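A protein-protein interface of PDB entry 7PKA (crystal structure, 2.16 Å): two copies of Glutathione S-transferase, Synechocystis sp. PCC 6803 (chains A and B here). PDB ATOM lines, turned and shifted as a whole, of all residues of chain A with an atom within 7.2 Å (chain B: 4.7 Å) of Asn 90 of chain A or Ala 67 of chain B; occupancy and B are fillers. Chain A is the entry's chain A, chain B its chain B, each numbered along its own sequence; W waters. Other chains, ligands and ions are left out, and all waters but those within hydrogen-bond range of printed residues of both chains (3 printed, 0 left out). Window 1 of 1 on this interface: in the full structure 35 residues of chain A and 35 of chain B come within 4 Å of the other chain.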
ATOM      1  N   GLY A  66     -19.818  12.575  -6.273  1.00  0.00           N
ATOM      2  CA  GLY A  66     -20.088  12.293  -7.676  1.00  0.00           C
ATOM      3  C   GLY A  66     -20.801  10.980  -7.882  1.00  0.00           C
ATOM      4  O   GLY A  66     -21.767  10.913  -8.641  1.00  0.00           O
ATOM      5  N   LEU A  70     -24.668  10.329  -9.338  1.00  0.00           N
ATOM      6  CA  LEU A  70     -24.946   9.369 -10.417  1.00  0.00           C
ATOM      7  C   LEU A  70     -25.943   8.299  -9.992  1.00  0.00           C
ATOM      8  O   LEU A  70     -26.871   8.007 -10.743  1.00  0.00           O
ATOM      9  CB  LEU A  70     -23.661   8.704 -10.928  1.00  0.00           C
ATOM     10  CG  LEU A  70     -22.713   9.655 -11.620  1.00  0.00           C
ATOM     11  CD1 LEU A  70     -21.322   9.039 -11.778  1.00  0.00           C
ATOM     12  CD2 LEU A  70     -23.284  10.089 -12.945  1.00  0.00           C
ATOM     13  N   GLU A  74     -29.716   7.766 -11.607  1.00  0.00           N
ATOM     14  CA  GLU A  74     -30.085   6.478 -12.157  1.00  0.00           C
ATOM     15  C   GLU A  74     -31.356   5.966 -11.481  1.00  0.00           C
ATOM     16  O   GLU A  74     -32.293   5.568 -12.166  1.00  0.00           O
ATOM     17  CB  GLU A  74     -28.933   5.492 -11.950  1.00  0.00           C
ATOM     18  CG  GLU A  74     -28.990   4.290 -12.864  1.00  0.00           C
ATOM     19  CD  GLU A  74     -27.698   3.498 -12.920  1.00  0.00           C
ATOM     20  OE1 GLU A  74     -26.627   4.059 -12.592  1.00  0.00           O
ATOM     21  OE2 GLU A  74     -27.763   2.308 -13.301  1.00  0.00           O
ATOM     22  N   ILE A  79     -31.867   9.190 -16.661  1.00  0.00           N
ATOM     23  CA  ILE A  79     -30.885   8.882 -17.715  1.00  0.00           C
ATOM     24  C   ILE A  79     -31.497   7.825 -18.650  1.00  0.00           C
ATOM     25  O   ILE A  79     -32.030   6.836 -18.153  1.00  0.00           O
ATOM     26  CB  ILE A  79     -29.523   8.400 -17.113  1.00  0.00           C
ATOM     27  CG1 ILE A  79     -29.066   9.295 -15.945  1.00  0.00           C
ATOM     28  CG2 ILE A  79     -28.444   8.308 -18.190  1.00  0.00           C
ATOM     29  CD1 ILE A  79     -27.900   8.833 -15.205  1.00  0.00           C
ATOM     30  N   ALA A  83     -25.315   2.176 -21.802  1.00  0.00           N
ATOM     31  CA  ALA A  83     -23.958   2.504 -21.353  1.00  0.00           C
ATOM     32  C   ALA A  83     -23.446   3.853 -21.890  1.00  0.00           C
ATOM     33  O   ALA A  83     -22.772   4.547 -21.150  1.00  0.00           O
ATOM     34  CB  ALA A  83     -22.985   1.389 -21.700  1.00  0.00           C
ATOM     35  N   GLN A  84     -23.840   4.261 -23.113  1.00  0.00           N
ATOM     36  CA  GLN A  84     -23.400   5.536 -23.685  1.00  0.00           C
ATOM     37  C   GLN A  84     -24.063   6.736 -23.050  1.00  0.00           C
ATOM     38  O   GLN A  84     -23.419   7.766 -22.878  1.00  0.00           O
ATOM     39  CB  GLN A  84     -23.561   5.559 -25.210  1.00  0.00           C
ATOM     40  CG  GLN A  84     -22.637   4.559 -25.893  1.00  0.00           C
ATOM     41  CD  GLN A  84     -22.619   4.643 -27.405  1.00  0.00           C
ATOM     42  OE1 GLN A  84     -23.369   5.403 -28.030  1.00  0.00           O
ATOM     43  NE2 GLN A  84     -21.742   3.860 -28.024  1.00  0.00           N
ATOM     44  N   ALA A  85     -25.334   6.601 -22.672  1.00  0.00           N
ATOM     45  CA  ALA A  85     -26.082   7.659 -22.024  1.00  0.00           C
ATOM     46  C   ALA A  85     -25.566   7.878 -20.619  1.00  0.00           C
ATOM     47  O   ALA A  85     -25.436   9.027 -20.198  1.00  0.00           O
ATOM     48  CB  ALA A  85     -27.561   7.304 -21.981  1.00  0.00           C
ATOM     49  N   ARG A  86     -25.255   6.795 -19.891  1.00  0.00           N
ATOM     50  CA  ARG A  86     -24.688   6.920 -18.553  1.00  0.00           C
ATOM     51  C   ARG A  86     -23.272   7.455 -18.640  1.00  0.00           C
ATOM     52  O   ARG A  86     -22.904   8.294 -17.825  1.00  0.00           O
ATOM     53  CB  ARG A  86     -24.670   5.582 -17.824  1.00  0.00           C
ATOM     54  CG  ARG A  86     -25.993   5.251 -17.177  1.00  0.00           C
ATOM     55  CD  ARG A  86     -25.855   4.031 -16.288  1.00  0.00           C
ATOM     56  NE  ARG A  86     -25.432   2.837 -17.025  1.00  0.00           N
ATOM     57  CZ  ARG A  86     -26.268   2.032 -17.674  1.00  0.00           C
ATOM     58  NH1 ARG A  86     -27.566   2.308 -17.722  1.00  0.00           N
ATOM     59  NH2 ARG A  86     -25.812   0.953 -18.297  1.00  0.00           N
ATOM     60  N   ALA A  87     -22.495   7.019 -19.655  1.00  0.00           N
ATOM     61  CA  ALA A  87     -21.118   7.485 -19.852  1.00  0.00           C
ATOM     62  C   ALA A  87     -21.051   8.988 -20.000  1.00  0.00           C
ATOM     63  O   ALA A  87     -20.167   9.607 -19.419  1.00  0.00           O
ATOM     64  CB  ALA A  87     -20.492   6.810 -21.076  1.00  0.00           C
ATOM     65  N   LEU A  88     -21.972   9.589 -20.763  1.00  0.00           N
ATOM     66  CA  LEU A  88     -21.956  11.043 -20.922  1.00  0.00           C
ATOM     67  C   LEU A  88     -22.207  11.760 -19.599  1.00  0.00           C
ATOM     68  O   LEU A  88     -21.550  12.754 -19.326  1.00  0.00           O
ATOM     69  CB  LEU A  88     -22.887  11.519 -22.029  1.00  0.00           C
ATOM     70  CG  LEU A  88     -22.530  10.989 -23.434  1.00  0.00           C
ATOM     71  CD1 LEU A  88     -23.491  11.555 -24.475  1.00  0.00           C
ATOM     72  CD2 LEU A  88     -21.045  11.312 -23.828  1.00  0.00           C
ATOM     73  N   VAL A  89     -23.085  11.233 -18.751  1.00  0.00           N
ATOM     74  CA  VAL A  89     -23.324  11.828 -17.425  1.00  0.00           C
ATOM     75  C   VAL A  89     -22.088  11.598 -16.517  1.00  0.00           C
ATOM     76  O   VAL A  89     -21.660  12.507 -15.821  1.00  0.00           O
ATOM     77  CB  VAL A  89     -24.639  11.280 -16.807  1.00  0.00           C
ATOM     78  CG1 VAL A  89     -24.921  11.939 -15.461  1.00  0.00           C
ATOM     79  CG2 VAL A  89     -25.817  11.495 -17.761  1.00  0.00           C
ATOM     80  N   ASN A  90     -21.506  10.383 -16.541  1.00  0.00           N
ATOM     81  CA  ASN A  90     -20.290  10.036 -15.787  1.00  0.00           C
ATOM     82  C   ASN A  90     -19.149  10.997 -16.170  1.00  0.00           C
ATOM     83  O   ASN A  90     -18.452  11.537 -15.312  1.00  0.00           O
ATOM     84  CB  ASN A  90     -19.863   8.594 -16.084  1.00  0.00           C
ATOM     85  CG  ASN A  90     -20.838   7.503 -15.660  1.00  0.00           C
ATOM     86  OD1 ASN A  90     -21.793   7.729 -14.907  1.00  0.00           O
ATOM     87  ND2 ASN A  90     -20.629   6.277 -16.148  1.00  0.00           N
ATOM     88  N   GLN A  91     -19.017  11.300 -17.466  1.00  0.00           N
ATOM     89  CA  GLN A  91     -17.997  12.238 -17.961  1.00  0.00           C
ATOM     90  C   GLN A  91     -18.057  13.580 -17.262  1.00  0.00           C
ATOM     91  O   GLN A  91     -17.043  14.069 -16.753  1.00  0.00           O
ATOM     92  CB  GLN A  91     -18.136  12.379 -19.494  1.00  0.00           C
ATOM     93  CG  GLN A  91     -17.477  13.582 -20.140  1.00  0.00           C
ATOM     94  CD  GLN A  91     -17.987  13.646 -21.553  1.00  0.00           C
ATOM     95  OE1 GLN A  91     -17.476  12.952 -22.425  1.00  0.00           O
ATOM     96  NE2 GLN A  91     -19.051  14.426 -21.787  1.00  0.00           N
ATOM     97  N   TRP A  92     -19.235  14.164 -17.218  1.00  0.00           N
ATOM     98  CA  TRP A  92     -19.410  15.471 -16.609  1.00  0.00           C
ATOM     99  C   TRP A  92     -19.232  15.437 -15.091  1.00  0.00           C
ATOM    100  O   TRP A  92     -18.698  16.397 -14.525  1.00  0.00           O
ATOM    101  CB  TRP A  92     -20.780  16.031 -16.985  1.00  0.00           C
ATOM    102  CG  TRP A  92     -20.837  16.522 -18.403  1.00  0.00           C
ATOM    103  CD1 TRP A  92     -21.474  15.928 -19.454  1.00  0.00           C
ATOM    104  CD2 TRP A  92     -20.220  17.707 -18.921  1.00  0.00           C
ATOM    105  NE1 TRP A  92     -21.285  16.673 -20.597  1.00  0.00           N
ATOM    106  CE2 TRP A  92     -20.527  17.776 -20.292  1.00  0.00           C
ATOM    107  CE3 TRP A  92     -19.462  18.740 -18.346  1.00  0.00           C
ATOM    108  CZ2 TRP A  92     -20.093  18.825 -21.101  1.00  0.00           C
ATOM    109  CZ3 TRP A  92     -19.017  19.767 -19.156  1.00  0.00           C
ATOM    110  CH2 TRP A  92     -19.355  19.814 -20.510  1.00  0.00           C
ATOM    111  N   ILE A  93     -19.636  14.331 -14.445  1.00  0.00           N
ATOM    112  CA  ILE A  93     -19.497  14.188 -12.991  1.00  0.00           C
ATOM    113  C   ILE A  93     -18.005  14.082 -12.635  1.00  0.00           C
ATOM    114  O   ILE A  93     -17.528  14.773 -11.738  1.00  0.00           O
ATOM    115  CB  ILE A  93     -20.398  13.042 -12.419  1.00  0.00           C
ATOM    116  CG1 ILE A  93     -21.788  13.590 -11.979  1.00  0.00           C
ATOM    117  CG2 ILE A  93     -19.730  12.342 -11.197  1.00  0.00           C
ATOM    118  CD1 ILE A  93     -22.605  14.186 -12.959  1.00  0.00           C
ATOM    119  N   LEU A  94     -17.256  13.301 -13.409  1.00  0.00           N
ATOM    120  CA  LEU A  94     -15.819  13.194 -13.213  1.00  0.00           C
ATOM    121  C   LEU A  94     -15.098  14.473 -13.506  1.00  0.00           C
ATOM    122  O   LEU A  94     -14.141  14.815 -12.805  1.00  0.00           O
ATOM    123  CB  LEU A  94     -15.259  12.036 -14.034  1.00  0.00           C
ATOM    124  CG  LEU A  94     -15.362  10.773 -13.200  1.00  0.00           C
ATOM    125  CD1 LEU A  94     -15.935   9.659 -13.970  1.00  0.00           C
ATOM    126  CD2 LEU A  94     -14.038  10.467 -12.512  1.00  0.00           C
ATOM    127  N   PHE A  95     -15.553  15.208 -14.541  1.00  0.00           N
ATOM    128  CA  PHE A  95     -14.960  16.491 -14.913  1.00  0.00           C
ATOM    129  C   PHE A  95     -15.166  17.485 -13.755  1.00  0.00           C
ATOM    130  O   PHE A  95     -14.219  18.137 -13.355  1.00  0.00           O
ATOM    131  CB  PHE A  95     -15.610  17.005 -16.206  1.00  0.00           C
ATOM    132  CG  PHE A  95     -15.424  18.482 -16.497  1.00  0.00           C
ATOM    133  CD1 PHE A  95     -14.264  18.945 -17.098  1.00  0.00           C
ATOM    134  CD2 PHE A  95     -16.427  19.396 -16.199  1.00  0.00           C
ATOM    135  CE1 PHE A  95     -14.100  20.296 -17.374  1.00  0.00           C
ATOM    136  CE2 PHE A  95     -16.254  20.745 -16.458  1.00  0.00           C
ATOM    137  CZ  PHE A  95     -15.089  21.186 -17.042  1.00  0.00           C
ATOM    138  N   ALA A  96     -16.390  17.576 -13.211  1.00  0.00           N
ATOM    139  CA  ALA A  96     -16.691  18.488 -12.087  1.00  0.00           C
ATOM    140  C   ALA A  96     -15.803  18.205 -10.874  1.00  0.00           C
ATOM    141  O   ALA A  96     -15.267  19.127 -10.263  1.00  0.00           O
ATOM    142  CB  ALA A  96     -18.163  18.376 -11.698  1.00  0.00           C
ATOM    143  N   VAL A 139     -26.022  16.902 -14.151  1.00  0.00           N
ATOM    144  CA  VAL A 139     -24.797  17.524 -14.640  1.00  0.00           C
ATOM    145  C   VAL A 139     -24.720  18.975 -14.184  1.00  0.00           C
ATOM    146  O   VAL A 139     -23.666  19.443 -13.742  1.00  0.00           O
ATOM    147  CB  VAL A 139     -24.650  17.367 -16.178  1.00  0.00           C
ATOM    148  CG1 VAL A 139     -23.507  18.234 -16.701  1.00  0.00           C
ATOM    149  CG2 VAL A 139     -24.442  15.899 -16.561  1.00  0.00           C
ATOM    150  N   LEU B  62     -16.114  10.213 -25.969  1.00  0.00           N
ATOM    151  CA  LEU B  62     -16.151  10.196 -24.515  1.00  0.00           C
ATOM    152  C   LEU B  62     -14.827  10.645 -23.966  1.00  0.00           C
ATOM    153  O   LEU B  62     -13.811  10.138 -24.393  1.00  0.00           O
ATOM    154  CB  LEU B  62     -16.443   8.761 -24.042  1.00  0.00           C
ATOM    155  CG  LEU B  62     -16.648   8.578 -22.527  1.00  0.00           C
ATOM    156  CD1 LEU B  62     -17.827   9.409 -22.009  1.00  0.00           C
ATOM    157  CD2 LEU B  62     -16.802   7.111 -22.185  1.00  0.00           C
ATOM    158  N   TRP B  63     -14.830  11.545 -22.974  1.00  0.00           N
ATOM    159  CA  TRP B  63     -13.596  12.006 -22.354  1.00  0.00           C
ATOM    160  C   TRP B  63     -13.698  11.858 -20.803  1.00  0.00           C
ATOM    161  O   TRP B  63     -14.758  11.509 -20.285  1.00  0.00           O
ATOM    162  CB  TRP B  63     -13.194  13.420 -22.853  1.00  0.00           C
ATOM    163  CG  TRP B  63     -14.335  14.396 -22.928  1.00  0.00           C
ATOM    164  CD1 TRP B  63     -15.205  14.566 -23.967  1.00  0.00           C
ATOM    165  CD2 TRP B  63     -14.770  15.290 -21.886  1.00  0.00           C
ATOM    166  NE1 TRP B  63     -16.119  15.550 -23.658  1.00  0.00           N
ATOM    167  CE2 TRP B  63     -15.893  15.987 -22.375  1.00  0.00           C
ATOM    168  CE3 TRP B  63     -14.332  15.547 -20.581  1.00  0.00           C
ATOM    169  CZ2 TRP B  63     -16.597  16.907 -21.594  1.00  0.00           C
ATOM    170  CZ3 TRP B  63     -15.001  16.496 -19.824  1.00  0.00           C
ATOM    171  CH2 TRP B  63     -16.140  17.136 -20.318  1.00  0.00           C
ATOM    172  N   GLU B  64     -12.580  12.059 -20.091  1.00  0.00           N
ATOM    173  CA  GLU B  64     -12.381  11.805 -18.655  1.00  0.00           C
ATOM    174  C   GLU B  64     -11.962  10.341 -18.586  1.00  0.00           C
ATOM    175  O   GLU B  64     -12.749   9.475 -18.926  1.00  0.00           O
ATOM    176  CB  GLU B  64     -13.615  12.093 -17.748  1.00  0.00           C
ATOM    177  CG  GLU B  64     -13.823  13.573 -17.395  1.00  0.00           C
ATOM    178  CD  GLU B  64     -12.634  14.245 -16.730  1.00  0.00           C
ATOM    179  OE1 GLU B  64     -12.006  13.612 -15.845  1.00  0.00           O
ATOM    180  OE2 GLU B  64     -12.318  15.401 -17.104  1.00  0.00           O
ATOM    181  N   SER B  65     -10.732  10.060 -18.178  1.00  0.00           N
ATOM    182  CA  SER B  65     -10.205   8.693 -18.082  1.00  0.00           C
ATOM    183  C   SER B  65     -11.094   7.807 -17.219  1.00  0.00           C
ATOM    184  O   SER B  65     -11.367   6.658 -17.595  1.00  0.00           O
ATOM    185  CB  SER B  65      -8.770   8.700 -17.547  1.00  0.00           C
ATOM    186  OG  SER B  65      -8.692   9.215 -16.227  1.00  0.00           O
ATOM    187  N   GLY B  66     -11.642   8.373 -16.139  1.00  0.00           N
ATOM    188  CA  GLY B  66     -12.518   7.600 -15.268  1.00  0.00           C
ATOM    189  C   GLY B  66     -13.797   7.147 -15.950  1.00  0.00           C
ATOM    190  O   GLY B  66     -14.228   6.013 -15.756  1.00  0.00           O
ATOM    191  N   ALA B  67     -14.430   8.035 -16.738  1.00  0.00           N
ATOM    192  CA  ALA B  67     -15.665   7.689 -17.459  1.00  0.00           C
ATOM    193  C   ALA B  67     -15.372   6.695 -18.579  1.00  0.00           C
ATOM    194  O   ALA B  67     -16.215   5.854 -18.868  1.00  0.00           O
ATOM    195  CB  ALA B  67     -16.336   8.936 -18.020  1.00  0.00           C
ATOM    196  N   ILE B  68     -14.177   6.768 -19.187  1.00  0.00           N
ATOM    197  CA  ILE B  68     -13.794   5.808 -20.207  1.00  0.00           C
ATOM    198  C   ILE B  68     -13.615   4.420 -19.563  1.00  0.00           C
ATOM    199  O   ILE B  68     -14.063   3.433 -20.138  1.00  0.00           O
ATOM    200  CB  ILE B  68     -12.502   6.250 -20.917  1.00  0.00           C
ATOM    201  CG1 ILE B  68     -12.693   7.610 -21.637  1.00  0.00           C
ATOM    202  CG2 ILE B  68     -11.984   5.144 -21.853  1.00  0.00           C
ATOM    203  CD1 ILE B  68     -11.345   8.201 -22.123  1.00  0.00           C
ATOM    204  N   LEU B  69     -12.950   4.332 -18.386  1.00  0.00           N
ATOM    205  CA  LEU B  69     -12.768   3.048 -17.678  1.00  0.00           C
ATOM    206  C   LEU B  69     -14.133   2.436 -17.361  1.00  0.00           C
ATOM    207  O   LEU B  69     -14.331   1.271 -17.652  1.00  0.00           O
ATOM    208  CB  LEU B  69     -11.994   3.236 -16.365  1.00  0.00           C
ATOM    209  CG  LEU B  69     -10.498   3.464 -16.483  1.00  0.00           C
ATOM    210  CD1 LEU B  69      -9.903   3.688 -15.116  1.00  0.00           C
ATOM    211  CD2 LEU B  69      -9.795   2.283 -17.249  1.00  0.00           C
ATOM    212  N   LEU B  70     -15.098   3.246 -16.858  1.00  0.00           N
ATOM    213  CA  LEU B  70     -16.453   2.756 -16.557  1.00  0.00           C
ATOM    214  C   LEU B  70     -17.201   2.323 -17.804  1.00  0.00           C
ATOM    215  O   LEU B  70     -17.924   1.321 -17.780  1.00  0.00           O
ATOM    216  CB  LEU B  70     -17.290   3.812 -15.816  1.00  0.00           C
ATOM    217  CG  LEU B  70     -16.693   4.299 -14.522  1.00  0.00           C
ATOM    218  CD1 LEU B  70     -17.482   5.472 -13.959  1.00  0.00           C
ATOM    219  CD2 LEU B  70     -16.594   3.166 -13.504  1.00  0.00           C
ATOM    220  N   TYR B  71     -17.051   3.082 -18.896  1.00  0.00           N
ATOM    221  CA  TYR B  71     -17.702   2.735 -20.155  1.00  0.00           C
ATOM    222  C   TYR B  71     -17.170   1.400 -20.680  1.00  0.00           C
ATOM    223  O   TYR B  71     -17.958   0.556 -21.065  1.00  0.00           O
ATOM    224  CB  TYR B  71     -17.504   3.845 -21.192  1.00  0.00           C
ATOM    225  CG  TYR B  71     -18.036   3.496 -22.566  1.00  0.00           C
ATOM    226  CD1 TYR B  71     -19.403   3.410 -22.803  1.00  0.00           C
ATOM    227  CD2 TYR B  71     -17.173   3.222 -23.620  1.00  0.00           C
ATOM    228  CE1 TYR B  71     -19.896   3.051 -24.051  1.00  0.00           C
ATOM    229  CE2 TYR B  71     -17.653   2.870 -24.876  1.00  0.00           C
ATOM    230  CZ  TYR B  71     -19.019   2.800 -25.092  1.00  0.00           C
ATOM    231  OH  TYR B  71     -19.507   2.493 -26.345  1.00  0.00           O
ATOM    232  N   ASN B  90     -18.312   3.124  -9.546  1.00  0.00           N
ATOM    233  CA  ASN B  90     -18.225   4.589  -9.728  1.00  0.00           C
ATOM    234  C   ASN B  90     -17.587   5.275  -8.521  1.00  0.00           C
ATOM    235  O   ASN B  90     -16.762   6.176  -8.677  1.00  0.00           O
ATOM    236  CB  ASN B  90     -19.619   5.207  -9.943  1.00  0.00           C
ATOM    237  CG  ASN B  90     -20.352   4.778 -11.199  1.00  0.00           C
ATOM    238  OD1 ASN B  90     -19.802   4.105 -12.063  1.00  0.00           O
ATOM    239  ND2 ASN B  90     -21.641   5.129 -11.316  1.00  0.00           N
HETATM  240  O   HOH W   1     -23.569   4.833 -13.752  1.00  0.00           O
HETATM  241  O   HOH W   2     -18.724   5.815 -18.116  1.00  0.00           O
HETATM  242  O   HOH W   3     -18.189  13.419 -25.124  1.00  0.00           O
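The backbone carbonyl oxygen (O) of Arg 86 of chain A lies close to the side-chain amide oxygen (OD1) of Asn 90 of chain A, at 3.2 Å.
NE2 of Gln 91 of chain A sits close to NE1 of Trp 92 of chain A (3.4 Å).
Leu 70 of chain A touches Asn 90 of chain B, and with the chains exchanged Asn 90 of chain A touches Leu 70 of chain B.
Among the printed residues, merely in contact across the chains: Gln 91 of chain A with Glu 64 of chain B (3.3 Å), Ala 87 of chain A with Leu 62 of chain B (3.5 Å), Leu 94 of chain A with Ala 67 of chain B (3.5 Å), Gln 91 of chain A with Leu 62 of chain B (3.6 Å), Phe 95 of chain A with Glu 64 of chain B (3.6 Å), Gln 91 of chain A with Ala 67 of chain B (3.6 Å), Phe 95 of chain A with Trp 63 of chain B (3.7 Å), Leu 94 of chain A with Gly 66 of chain B (3.8 Å), Leu 94 of chain A with Glu 64 of chain B (3.9 Å), Asn 90 of chain A with Leu 70 of chain B (3.9 Å), Ala 83 of chain A with Tyr 71 of chain B (3.9 Å), Asn 90 of chain A with Ala 67 of chain B (3.9 Å), Leu 70 of chain A with Asn 90 of chain B (3.95 Å) and Ala 87 of chain A with Tyr 71 of chain B (3.97 Å).
Printed residues of chain B within 4 Å of Ala 83 of chain A: Tyr 71 (3.9 Å).
Printed residues of chain B within 4 Å of Ala 87 of chain A: Leu 62 and Tyr 71.
Ile 93 of chain A touches none of the printed residues of chain B.
Printed residues of chain A within 4 Å of Trp 63 of chain B: Gln 91 (3.0 Å) and Phe 95 (3.7 Å).
Of the printed residues of chain A, Gly 66 of chain B touches Leu 94.
Of chain A, only Asn 90, Gln 91 and Leu 94 come within 4 Å of Ala 67 of chain B.
Of the printed residues of chain A, Tyr 71 of chain B touches Ala 83 (3.9 Å), Gln 84 (3.1 Å) and Ala 87 (3.97 Å).
The nearest residue of chain A that does not touch Ala 67 of chain B is Ala 87 of chain A (4.1 Å).
The nearest printed residue of chain B that does not touch Ala 83 of chain A is Leu 70 of chain B (6.4 Å).
Water W2 lies within hydrogen-bond range of the backbone carbonyl oxygen (O) of Ala 67 of chain B, the side-chain amide nitrogen (ND2) of Asn 90 of chain A and the backbone NH (N) of Tyr 71 of chain B.
Water W3 bridges OE1 of Gln 91 of chain A (2.8 Å) and NE1 of Trp 63 of chain B (3.3 Å).
Water W1 bridges the side-chain amide nitrogen (ND2) of Asn 90 of chain B (3.1 Å) and the side-chain carboxylate (OE1) of Glu 74 of chain A (3.4 Å).
OH of Tyr 71 of chain B sits at hydrogen-bond distance from NE2 of Gln 84 of chain A (3.1 Å).
The side-chain amide oxygen (OE1) of Gln 91 of chain A lies within hydrogen-bond range of the backbone NH (N) of Trp 63 of chain B (3.0 Å).
Of the 19 printed residues of chain A, 8 touch a printed residue of chain B.
Hydrophobic or aromatic side chains of chain A within 4 Å of the printed part of chain B: Leu 70, Ala 87, Leu 94 and Phe 95.
Printed residues of chain B that touch a printed residue of chain A: Leu 62, Trp 63, Glu 64, Gly 66, Ala 67, Leu 70, Tyr 71 and Asn 90.
Hydrophobic or aromatic side chains of chain B that line the printed part of chain A: Leu 62, Trp 63, Ala 67, Leu 70 and Tyr 71.
Along chain B the printed residues that touch a printed residue of chain A span positions 62 to 90.
Among the printed residues, 16 pairs touch across the chains.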
